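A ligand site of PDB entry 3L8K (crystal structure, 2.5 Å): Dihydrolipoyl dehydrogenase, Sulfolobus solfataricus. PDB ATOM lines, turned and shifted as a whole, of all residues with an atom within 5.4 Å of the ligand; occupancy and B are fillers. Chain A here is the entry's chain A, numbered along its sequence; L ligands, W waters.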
ATOM      1  N   ILE A  10      -6.964  -6.223  -2.262  1.00  0.00           N
ATOM      2  CA  ILE A  10      -8.360  -6.344  -1.959  1.00  0.00           C
ATOM      3  C   ILE A  10      -8.594  -6.404  -0.422  1.00  0.00           C
ATOM      4  O   ILE A  10      -8.288  -7.413   0.253  1.00  0.00           O
ATOM      5  CB  ILE A  10      -8.919  -7.604  -2.610  1.00  0.00           C
ATOM      6  CG1 ILE A  10      -8.615  -7.580  -4.119  1.00  0.00           C
ATOM      7  CG2 ILE A  10     -10.430  -7.726  -2.346  1.00  0.00           C
ATOM      8  CD1 ILE A  10      -9.001  -8.834  -4.841  1.00  0.00           C
ATOM      9  N   GLY A  11      -9.126  -5.319   0.105  1.00  0.00           N
ATOM     10  CA  GLY A  11      -9.374  -5.180   1.546  1.00  0.00           C
ATOM     11  C   GLY A  11      -8.369  -4.269   2.192  1.00  0.00           C
ATOM     12  O   GLY A  11      -7.172  -4.357   1.887  1.00  0.00           O
ATOM     13  N   ALA A  12      -8.830  -3.407   3.104  1.00  0.00           N
ATOM     14  CA  ALA A  12      -7.995  -2.401   3.724  1.00  0.00           C
ATOM     15  C   ALA A  12      -7.867  -2.573   5.223  1.00  0.00           C
ATOM     16  O   ALA A  12      -7.628  -1.610   5.970  1.00  0.00           O
ATOM     17  CB  ALA A  12      -8.556  -1.005   3.399  1.00  0.00           C
ATOM     18  N   GLY A  13      -8.046  -3.779   5.697  1.00  0.00           N
ATOM     19  CA  GLY A  13      -7.650  -4.064   7.076  1.00  0.00           C
ATOM     20  C   GLY A  13      -6.138  -4.253   7.243  1.00  0.00           C
ATOM     21  O   GLY A  13      -5.362  -3.966   6.342  1.00  0.00           O
ATOM     22  N   GLY A  14      -5.742  -4.770   8.403  1.00  0.00           N
ATOM     23  CA  GLY A  14      -4.342  -5.067   8.692  1.00  0.00           C
ATOM     24  C   GLY A  14      -3.674  -5.911   7.645  1.00  0.00           C
ATOM     25  O   GLY A  14      -2.571  -5.592   7.197  1.00  0.00           O
ATOM     26  N   ALA A  15      -4.340  -6.981   7.245  1.00  0.00           N
ATOM     27  CA  ALA A  15      -3.877  -7.851   6.159  1.00  0.00           C
ATOM     28  C   ALA A  15      -3.526  -7.136   4.834  1.00  0.00           C
ATOM     29  O   ALA A  15      -2.792  -7.673   4.012  1.00  0.00           O
ATOM     30  CB  ALA A  15      -4.916  -8.906   5.910  1.00  0.00           C
ATOM     31  N   GLY A  16      -4.026  -5.910   4.656  1.00  0.00           N
ATOM     32  CA  GLY A  16      -3.942  -5.227   3.380  1.00  0.00           C
ATOM     33  C   GLY A  16      -3.098  -3.976   3.402  1.00  0.00           C
ATOM     34  O   GLY A  16      -2.180  -3.838   2.607  1.00  0.00           O
ATOM     35  N   ALA A  33      -8.816  -1.276  -2.506  1.00  0.00           N
ATOM     36  CA  ALA A  33     -10.224  -0.977  -2.392  1.00  0.00           C
ATOM     37  C   ALA A  33     -10.846  -1.711  -1.194  1.00  0.00           C
ATOM     38  O   ALA A  33     -10.469  -2.834  -0.920  1.00  0.00           O
ATOM     39  CB  ALA A  33     -10.917  -1.387  -3.674  1.00  0.00           C
ATOM     40  N   ASP A  34     -11.766  -1.057  -0.474  1.00  0.00           N
ATOM     41  CA  ASP A  34     -12.552  -1.643   0.615  1.00  0.00           C
ATOM     42  C   ASP A  34     -13.915  -0.929   0.687  1.00  0.00           C
ATOM     43  O   ASP A  34     -13.956   0.283   0.750  1.00  0.00           O
ATOM     44  CB  ASP A  34     -11.803  -1.435   1.943  1.00  0.00           C
ATOM     45  CG  ASP A  34     -12.323  -2.323   3.077  1.00  0.00           C
ATOM     46  OD1 ASP A  34     -13.523  -2.324   3.358  1.00  0.00           O
ATOM     47  OD2 ASP A  34     -11.502  -3.001   3.747  1.00  0.00           O
ATOM     48  N   PRO A  35     -15.025  -1.681   0.746  1.00  0.00           N
ATOM     49  CA  PRO A  35     -16.369  -1.135   0.925  1.00  0.00           C
ATOM     50  C   PRO A  35     -16.566  -0.170   2.114  1.00  0.00           C
ATOM     51  O   PRO A  35     -17.425   0.716   2.041  1.00  0.00           O
ATOM     52  CB  PRO A  35     -17.193  -2.379   1.205  1.00  0.00           C
ATOM     53  CG  PRO A  35     -16.504  -3.440   0.563  1.00  0.00           C
ATOM     54  CD  PRO A  35     -15.067  -3.145   0.668  1.00  0.00           C
ATOM     55  N   LYS A  36     -15.866  -0.375   3.212  1.00  0.00           N
ATOM     56  CA  LYS A  36     -15.980   0.556   4.312  1.00  0.00           C
ATOM     57  C   LYS A  36     -15.471   1.950   3.956  1.00  0.00           C
ATOM     58  O   LYS A  36     -15.855   2.935   4.583  1.00  0.00           O
ATOM     59  CB  LYS A  36     -15.169   0.077   5.511  1.00  0.00           C
ATOM     60  CG  LYS A  36     -15.766  -1.134   6.234  1.00  0.00           C
ATOM     61  CD  LYS A  36     -14.903  -1.477   7.446  1.00  0.00           C
ATOM     62  CE  LYS A  36     -14.869  -2.982   7.677  1.00  0.00           C
ATOM     63  NZ  LYS A  36     -16.188  -3.512   8.048  1.00  0.00           N
ATOM     64  N   GLY A  40      -8.412  -0.260   8.457  1.00  0.00           N
ATOM     65  CA  GLY A  40      -8.455  -0.949   9.762  1.00  0.00           C
ATOM     66  C   GLY A  40      -9.297  -2.222   9.764  1.00  0.00           C
ATOM     67  O   GLY A  40      -9.162  -3.065  10.670  1.00  0.00           O
ATOM     68  N   GLY A  41     -10.173  -2.328   8.773  1.00  0.00           N
ATOM     69  CA  GLY A  41     -11.006  -3.464   8.577  1.00  0.00           C
ATOM     70  C   GLY A  41     -11.965  -3.690   9.715  1.00  0.00           C
ATOM     71  O   GLY A  41     -12.278  -2.779  10.503  1.00  0.00           O
ATOM     72  N   ASN A  42     -12.412  -4.919   9.810  1.00  0.00           N
ATOM     73  CA  ASN A  42     -13.323  -5.292  10.849  1.00  0.00           C
ATOM     74  C   ASN A  42     -12.728  -5.181  12.261  1.00  0.00           C
ATOM     75  O   ASN A  42     -13.447  -4.850  13.220  1.00  0.00           O
ATOM     76  CB  ASN A  42     -13.828  -6.704  10.548  1.00  0.00           C
ATOM     77  CG  ASN A  42     -14.624  -6.734   9.275  1.00  0.00           C
ATOM     78  OD1 ASN A  42     -15.467  -5.837   9.064  1.00  0.00           O
ATOM     79  ND2 ASN A  42     -14.365  -7.722   8.396  1.00  0.00           N
ATOM     80  N   CYS A  43     -11.437  -5.428  12.380  1.00  0.00           N
ATOM     81  CA  CYS A  43     -10.806  -5.351  13.686  1.00  0.00           C
ATOM     82  C   CYS A  43     -10.917  -3.951  14.327  1.00  0.00           C
ATOM     83  O   CYS A  43     -11.236  -3.818  15.518  1.00  0.00           O
ATOM     84  CB  CYS A  43      -9.352  -5.804  13.585  1.00  0.00           C
ATOM     85  SG  CYS A  43      -8.483  -5.404  15.095  1.00  0.00           S
ATOM     86  N   GLY A 109     -15.103   0.615  -2.366  1.00  0.00           N
ATOM     87  CA  GLY A 109     -15.801  -0.285  -3.265  1.00  0.00           C
ATOM     88  C   GLY A 109     -15.364  -1.723  -3.060  1.00  0.00           C
ATOM     89  O   GLY A 109     -14.557  -1.996  -2.164  1.00  0.00           O
ATOM     90  N   TYR A 110     -15.890  -2.633  -3.877  1.00  0.00           N
ATOM     91  CA  TYR A 110     -15.637  -4.085  -3.828  1.00  0.00           C
ATOM     92  C   TYR A 110     -14.870  -4.506  -5.080  1.00  0.00           C
ATOM     93  O   TYR A 110     -15.261  -4.092  -6.159  1.00  0.00           O
ATOM     94  CB  TYR A 110     -16.963  -4.869  -3.898  1.00  0.00           C
ATOM     95  CG  TYR A 110     -17.907  -4.764  -2.722  1.00  0.00           C
ATOM     96  CD1 TYR A 110     -17.805  -5.645  -1.649  1.00  0.00           C
ATOM     97  CD2 TYR A 110     -18.945  -3.847  -2.707  1.00  0.00           C
ATOM     98  CE1 TYR A 110     -18.672  -5.567  -0.580  1.00  0.00           C
ATOM     99  CE2 TYR A 110     -19.825  -3.769  -1.644  1.00  0.00           C
ATOM    100  CZ  TYR A 110     -19.680  -4.625  -0.587  1.00  0.00           C
ATOM    101  OH  TYR A 110     -20.533  -4.557   0.484  1.00  0.00           O
ATOM    102  N   VAL A 111     -13.863  -5.372  -4.950  1.00  0.00           N
ATOM    103  CA  VAL A 111     -13.126  -5.874  -6.110  1.00  0.00           C
ATOM    104  C   VAL A 111     -13.670  -7.222  -6.541  1.00  0.00           C
ATOM    105  O   VAL A 111     -13.935  -8.072  -5.711  1.00  0.00           O
ATOM    106  CB  VAL A 111     -11.657  -5.992  -5.775  1.00  0.00           C
ATOM    107  CG1 VAL A 111     -10.887  -6.406  -6.968  1.00  0.00           C
ATOM    108  CG2 VAL A 111     -11.157  -4.650  -5.274  1.00  0.00           C
ATOM    109  N   LYS A 112     -13.899  -7.367  -7.848  1.00  0.00           N
ATOM    110  CA  LYS A 112     -14.262  -8.617  -8.474  1.00  0.00           C
ATOM    111  C   LYS A 112     -13.069  -8.988  -9.324  1.00  0.00           C
ATOM    112  O   LYS A 112     -12.451  -8.131  -9.926  1.00  0.00           O
ATOM    113  CB  LYS A 112     -15.514  -8.450  -9.345  1.00  0.00           C
ATOM    114  N   ALA A 139      -6.911  -9.752   0.712  1.00  0.00           N
ATOM    115  CA  ALA A 139      -6.835  -9.425   2.124  1.00  0.00           C
ATOM    116  C   ALA A 139      -8.231  -9.138   2.581  1.00  0.00           C
ATOM    117  O   ALA A 139      -8.430  -8.192   3.308  1.00  0.00           O
ATOM    118  CB  ALA A 139      -5.981  -8.194   2.339  1.00  0.00           C
ATOM    119  N   SER A 140      -9.175  -9.962   2.153  1.00  0.00           N
ATOM    120  CA  SER A 140     -10.599  -9.699   2.292  1.00  0.00           C
ATOM    121  C   SER A 140     -11.205 -10.152   3.610  1.00  0.00           C
ATOM    122  O   SER A 140     -12.373  -9.945   3.861  1.00  0.00           O
ATOM    123  CB  SER A 140     -11.339 -10.366   1.138  1.00  0.00           C
ATOM    124  OG  SER A 140     -10.793 -11.664   0.861  1.00  0.00           O
ATOM    125  N   GLY A 141     -10.401 -10.776   4.445  1.00  0.00           N
ATOM    126  CA  GLY A 141     -10.797 -10.995   5.839  1.00  0.00           C
ATOM    127  C   GLY A 141     -11.874 -12.033   6.020  1.00  0.00           C
ATOM    128  O   GLY A 141     -11.959 -12.998   5.284  1.00  0.00           O
ATOM    129  N   ALA A 142     -12.709 -11.827   7.016  1.00  0.00           N
ATOM    130  CA  ALA A 142     -13.715 -12.804   7.378  1.00  0.00           C
ATOM    131  C   ALA A 142     -14.961 -12.071   7.814  1.00  0.00           C
ATOM    132  O   ALA A 142     -14.916 -10.855   8.018  1.00  0.00           O
ATOM    133  CB  ALA A 142     -13.189 -13.685   8.527  1.00  0.00           C
ATOM    134  N   ARG A 270     -16.197 -16.763  12.995  1.00  0.00           N
ATOM    135  CA  ARG A 270     -16.214 -15.978  11.773  1.00  0.00           C
ATOM    136  C   ARG A 270     -15.820 -16.905  10.643  1.00  0.00           C
ATOM    137  O   ARG A 270     -15.282 -17.980  10.890  1.00  0.00           O
ATOM    138  CB  ARG A 270     -15.264 -14.797  11.888  1.00  0.00           C
ATOM    139  CG  ARG A 270     -15.459 -13.986  13.173  1.00  0.00           C
ATOM    140  CD  ARG A 270     -14.613 -12.702  13.197  1.00  0.00           C
ATOM    141  NE  ARG A 270     -15.425 -11.505  12.972  1.00  0.00           N
ATOM    142  CZ  ARG A 270     -15.441 -10.772  11.865  1.00  0.00           C
ATOM    143  NH1 ARG A 270     -14.654 -11.061  10.841  1.00  0.00           N
ATOM    144  NH2 ARG A 270     -16.241  -9.711  11.797  1.00  0.00           N
ATOM    145  N   VAL A 273     -13.982 -14.640   3.889  1.00  0.00           N
ATOM    146  CA  VAL A 273     -14.715 -13.954   2.849  1.00  0.00           C
ATOM    147  C   VAL A 273     -13.885 -14.042   1.573  1.00  0.00           C
ATOM    148  O   VAL A 273     -12.755 -13.526   1.502  1.00  0.00           O
ATOM    149  CB  VAL A 273     -14.948 -12.491   3.240  1.00  0.00           C
ATOM    150  CG1 VAL A 273     -15.463 -11.673   2.062  1.00  0.00           C
ATOM    151  CG2 VAL A 273     -15.868 -12.407   4.445  1.00  0.00           C
ATOM    152  N   PRO A 275     -13.494 -13.180  -2.367  1.00  0.00           N
ATOM    153  CA  PRO A 275     -14.012 -12.247  -3.384  1.00  0.00           C
ATOM    154  C   PRO A 275     -14.612 -12.918  -4.623  1.00  0.00           C
ATOM    155  O   PRO A 275     -14.153 -13.974  -5.067  1.00  0.00           O
ATOM    156  CB  PRO A 275     -12.794 -11.440  -3.811  1.00  0.00           C
ATOM    157  CG  PRO A 275     -11.624 -11.991  -3.055  1.00  0.00           C
ATOM    158  CD  PRO A 275     -12.042 -13.149  -2.238  1.00  0.00           C
ATOM    159  N   GLU A 276     -15.591 -12.249  -5.207  1.00  0.00           N
ATOM    160  CA  GLU A 276     -16.192 -12.693  -6.456  1.00  0.00           C
ATOM    161  C   GLU A 276     -15.140 -12.862  -7.526  1.00  0.00           C
ATOM    162  O   GLU A 276     -14.291 -11.978  -7.767  1.00  0.00           O
ATOM    163  CB  GLU A 276     -17.246 -11.680  -6.919  1.00  0.00           C
ATOM    164  CG  GLU A 276     -18.314 -12.247  -7.823  1.00  0.00           C
ATOM    165  CD  GLU A 276     -19.231 -11.152  -8.416  1.00  0.00           C
ATOM    166  OE1 GLU A 276     -19.914 -11.447  -9.439  1.00  0.00           O
ATOM    167  OE2 GLU A 276     -19.239 -10.008  -7.859  1.00  0.00           O
ATOM    168  N   THR A 306      -3.536 -12.876   2.433  1.00  0.00           N
ATOM    169  CA  THR A 306      -3.017 -12.528   3.764  1.00  0.00           C
ATOM    170  C   THR A 306      -4.194 -12.335   4.740  1.00  0.00           C
ATOM    171  O   THR A 306      -5.320 -12.053   4.337  1.00  0.00           O
ATOM    172  CB  THR A 306      -2.204 -11.228   3.670  1.00  0.00           C
ATOM    173  OG1 THR A 306      -3.066 -10.160   3.274  1.00  0.00           O
ATOM    174  CG2 THR A 306      -1.075 -11.357   2.611  1.00  0.00           C
ATOM    175  N   GLY A 307      -3.948 -12.502   6.028  1.00  0.00           N
ATOM    176  CA  GLY A 307      -4.978 -12.277   7.034  1.00  0.00           C
ATOM    177  C   GLY A 307      -6.032 -13.352   7.135  1.00  0.00           C
ATOM    178  O   GLY A 307      -5.836 -14.428   6.640  1.00  0.00           O
ATOM    179  N   ASP A 308      -7.163 -13.038   7.746  1.00  0.00           N
ATOM    180  CA  ASP A 308      -8.191 -14.033   7.996  1.00  0.00           C
ATOM    181  C   ASP A 308      -8.689 -14.745   6.737  1.00  0.00           C
ATOM    182  O   ASP A 308      -9.258 -15.805   6.830  1.00  0.00           O
ATOM    183  CB  ASP A 308      -9.418 -13.442   8.697  1.00  0.00           C
ATOM    184  CG  ASP A 308      -9.103 -12.683  10.005  1.00  0.00           C
ATOM    185  OD1 ASP A 308      -7.977 -12.776  10.576  1.00  0.00           O
ATOM    186  OD2 ASP A 308     -10.018 -11.931  10.467  1.00  0.00           O
ATOM    187  N   ALA A 309      -8.480 -14.197   5.555  1.00  0.00           N
ATOM    188  CA  ALA A 309      -8.904 -14.851   4.316  1.00  0.00           C
ATOM    189  C   ALA A 309      -8.223 -16.197   4.141  1.00  0.00           C
ATOM    190  O   ALA A 309      -8.781 -17.070   3.498  1.00  0.00           O
ATOM    191  CB  ALA A 309      -8.604 -13.943   3.087  1.00  0.00           C
ATOM    192  N   TYR A 316      -5.163 -10.029  14.433  1.00  0.00           N
ATOM    193  CA  TYR A 316      -4.732  -8.842  13.702  1.00  0.00           C
ATOM    194  C   TYR A 316      -3.188  -8.722  13.527  1.00  0.00           C
ATOM    195  O   TYR A 316      -2.681  -8.409  12.427  1.00  0.00           O
ATOM    196  CB  TYR A 316      -5.298  -7.592  14.365  1.00  0.00           C
ATOM    197  CG  TYR A 316      -4.793  -6.306  13.785  1.00  0.00           C
ATOM    198  CD1 TYR A 316      -5.479  -5.648  12.774  1.00  0.00           C
ATOM    199  CD2 TYR A 316      -3.615  -5.717  14.249  1.00  0.00           C
ATOM    200  CE1 TYR A 316      -5.014  -4.446  12.241  1.00  0.00           C
ATOM    201  CE2 TYR A 316      -3.164  -4.533  13.726  1.00  0.00           C
ATOM    202  CZ  TYR A 316      -3.868  -3.918  12.727  1.00  0.00           C
ATOM    203  OH  TYR A 316      -3.400  -2.747  12.215  1.00  0.00           O
ATOM    204  N   ALA A 319      -1.998 -10.957  10.832  1.00  0.00           N
ATOM    205  CA  ALA A 319      -2.422 -10.474   9.520  1.00  0.00           C
ATOM    206  C   ALA A 319      -1.459  -9.378   9.029  1.00  0.00           C
ATOM    207  O   ALA A 319      -1.076  -9.348   7.846  1.00  0.00           O
ATOM    208  CB  ALA A 319      -3.844  -9.934   9.589  1.00  0.00           C
HETATM  209  P1  LIG L   1      -7.824  -8.794   8.212  1.00  0.00           P
HETATM  210  O1  LIG L   1      -7.366  -7.495   7.586  1.00  0.00           O
HETATM  211  O2  LIG L   1      -7.484 -10.067   7.518  1.00  0.00           O
HETATM  212  O3  LIG L   1      -7.581  -8.873   9.719  1.00  0.00           O
HETATM  213  P2  LIG L   1     -10.574  -7.836   8.380  1.00  0.00           P
HETATM  214  O4  LIG L   1     -10.148  -7.024   9.590  1.00  0.00           O
HETATM  215  O5  LIG L   1     -11.845  -8.662   8.398  1.00  0.00           O
HETATM  216  O6  LIG L   1      -9.406  -8.897   7.952  1.00  0.00           O
HETATM  217  O7  LIG L   1     -10.710  -6.819   7.146  1.00  0.00           O
HETATM  218  C1  LIG L   1     -10.935  -7.266   5.819  1.00  0.00           C
HETATM  219  C2  LIG L   1     -11.508  -6.126   4.985  1.00  0.00           C
HETATM  220  O8  LIG L   1     -11.679  -6.590   3.642  1.00  0.00           O
HETATM  221  C3  LIG L   1     -12.882  -5.688   5.483  1.00  0.00           C
HETATM  222  O9  LIG L   1     -12.759  -4.320   5.868  1.00  0.00           O
HETATM  223  C4  LIG L   1     -13.850  -5.927   4.312  1.00  0.00           C
HETATM  224  O10 LIG L   1     -14.789  -4.858   4.081  1.00  0.00           O
HETATM  225  C5  LIG L   1     -12.897  -6.029   3.134  1.00  0.00           C
HETATM  226  N1  LIG L   1     -13.357  -6.825   1.976  1.00  0.00           N
HETATM  227  C6  LIG L   1     -13.989  -8.031   1.953  1.00  0.00           C
HETATM  228  N2  LIG L   1     -14.210  -8.410   0.673  1.00  0.00           N
HETATM  229  C7  LIG L   1     -13.707  -7.441  -0.137  1.00  0.00           C
HETATM  230  C8  LIG L   1     -13.613  -7.159  -1.603  1.00  0.00           C
HETATM  231  N3  LIG L   1     -14.070  -8.002  -2.542  1.00  0.00           N
HETATM  232  N4  LIG L   1     -13.019  -5.998  -2.004  1.00  0.00           N
HETATM  233  C9  LIG L   1     -12.518  -5.098  -1.126  1.00  0.00           C
HETATM  234  N5  LIG L   1     -12.597  -5.290   0.200  1.00  0.00           N
HETATM  235  C10 LIG L   1     -13.161  -6.399   0.737  1.00  0.00           C
HETATM  236  O   HOH W   1      -7.404  -6.427   5.122  1.00  0.00           O
HETATM  237  O   HOH W   2      -7.671 -11.495   5.029  1.00  0.00           O
HETATM  238  O   HOH W   3     -16.419  -9.525  -4.307  1.00  0.00           O
HETATM  239  O   HOH W   4      -8.071  -5.405  10.139  1.00  0.00           O
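Water W1 lies within hydrogen-bond range of O1 of the ligand (2.7 Å), O of Ala 139 (2.7 Å), N of Gly 13 (2.8 Å) and N of Gly 16 (3.4 Å). Water W4 lies within hydrogen-bond range of the backbone carbonyl oxygen of Gly 40, an oxygen (O4) of the ligand and the backbone NH of Gly 14. Water W3 lies within hydrogen-bond range of the backbone NH (N) of Glu 276 (3.0 Å), the backbone carbonyl oxygen (O) of Val 111 (3.2 Å) and a nitrogen (N3) of the ligand (3.3 Å).
A nitrogen (N5) of the ligand sits close to the backbone carbonyl oxygen (O) of Ala 33 (3.4 Å). The backbone carbonyl oxygen (O) of Ser 140 sits close to an oxygen (O8) of the ligand. Merely in contact with the ligand: Lys 36 (3.1 Å), Ile 10 (3.1 Å), Gly 141 (3.3 Å), Pro 35 (3.3 Å), Gly 41 (3.3 Å), Gly 307 (3.4 Å), Gly 13 (3.5 Å), Ala 142 (3.6 Å), Ala 139 (3.6 Å), Tyr 110 (3.7 Å), Val 273 (3.8 Å), Gly 109 (3.9 Å), Pro 275 (3.9 Å) and Ala 319 (3.9 Å). Hydrophobic or aromatic side chains that line the ligand: Ile 10, Ala 15, Pro 35, Val 111, Val 273, Pro 275 and Ala 319. The nearest printed residue that does not touch the ligand is Gly 40 (4.2 Å).
The side-chain amide nitrogen (ND2) of Asn 42 lies within hydrogen-bond range of the backbone carbonyl oxygen (O) of Ala 142 (3.2 Å). The backbone NH of Ala 139 sits at hydrogen-bond distance from the backbone carbonyl oxygen of Ile 10 (2.8 Å). OG1 of Thr 306 is in hydrogen-bond range of O of Ala 15. The side-chain carboxylate (OD2) of Asp 34 sits at hydrogen-bond distance from the backbone NH (N) of Ala 12 (2.8 Å). The backbone NH (N) of Gly 109 is in hydrogen-bond range of the backbone carbonyl oxygen (O) of Asp 34 (3.3 Å). N of Gly 11 lies within hydrogen-bond range of O of Ala 33, at 3.0 Å. The backbone carbonyl oxygen (O) of Ile 10 lies within hydrogen-bond range of the backbone NH (N) of Ser 140. NZ of Lys 36 lies within hydrogen-bond range of OD1 of Asn 42 (2.6 Å).
O2 of the ligand sits at hydrogen-bond distance from N of Asp 308 (3.0 Å). N3 of the ligand sits at hydrogen-bond distance from O of Val 111 (3.2 Å). A nitrogen (N4) of the ligand sits at hydrogen-bond distance from the backbone NH of Val 111 (3.1 Å). The backbone NH (N) of Ala 15 is in hydrogen-bond range of an oxygen (O1) of the ligand (3.1 Å). The backbone NH (N) of Gly 11 is in hydrogen-bond range of a nitrogen (N5) of the ligand, at 3.5 Å. O5 of the ligand sits at hydrogen-bond distance from ND2 of Asn 42 (2.7 Å). The backbone NH of Cys 43 sits at hydrogen-bond distance from an oxygen (O4) of the ligand (3.5 Å). N of Gly 14 sits at hydrogen-bond distance from O1 of the ligand, at 3.3 Å. The backbone NH (N) of Asn 42 sits at hydrogen-bond distance from an oxygen (O4) of the ligand (3.1 Å). OD2 of Asp 34 sits at hydrogen-bond distance from O9 of the ligand (2.8 Å).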
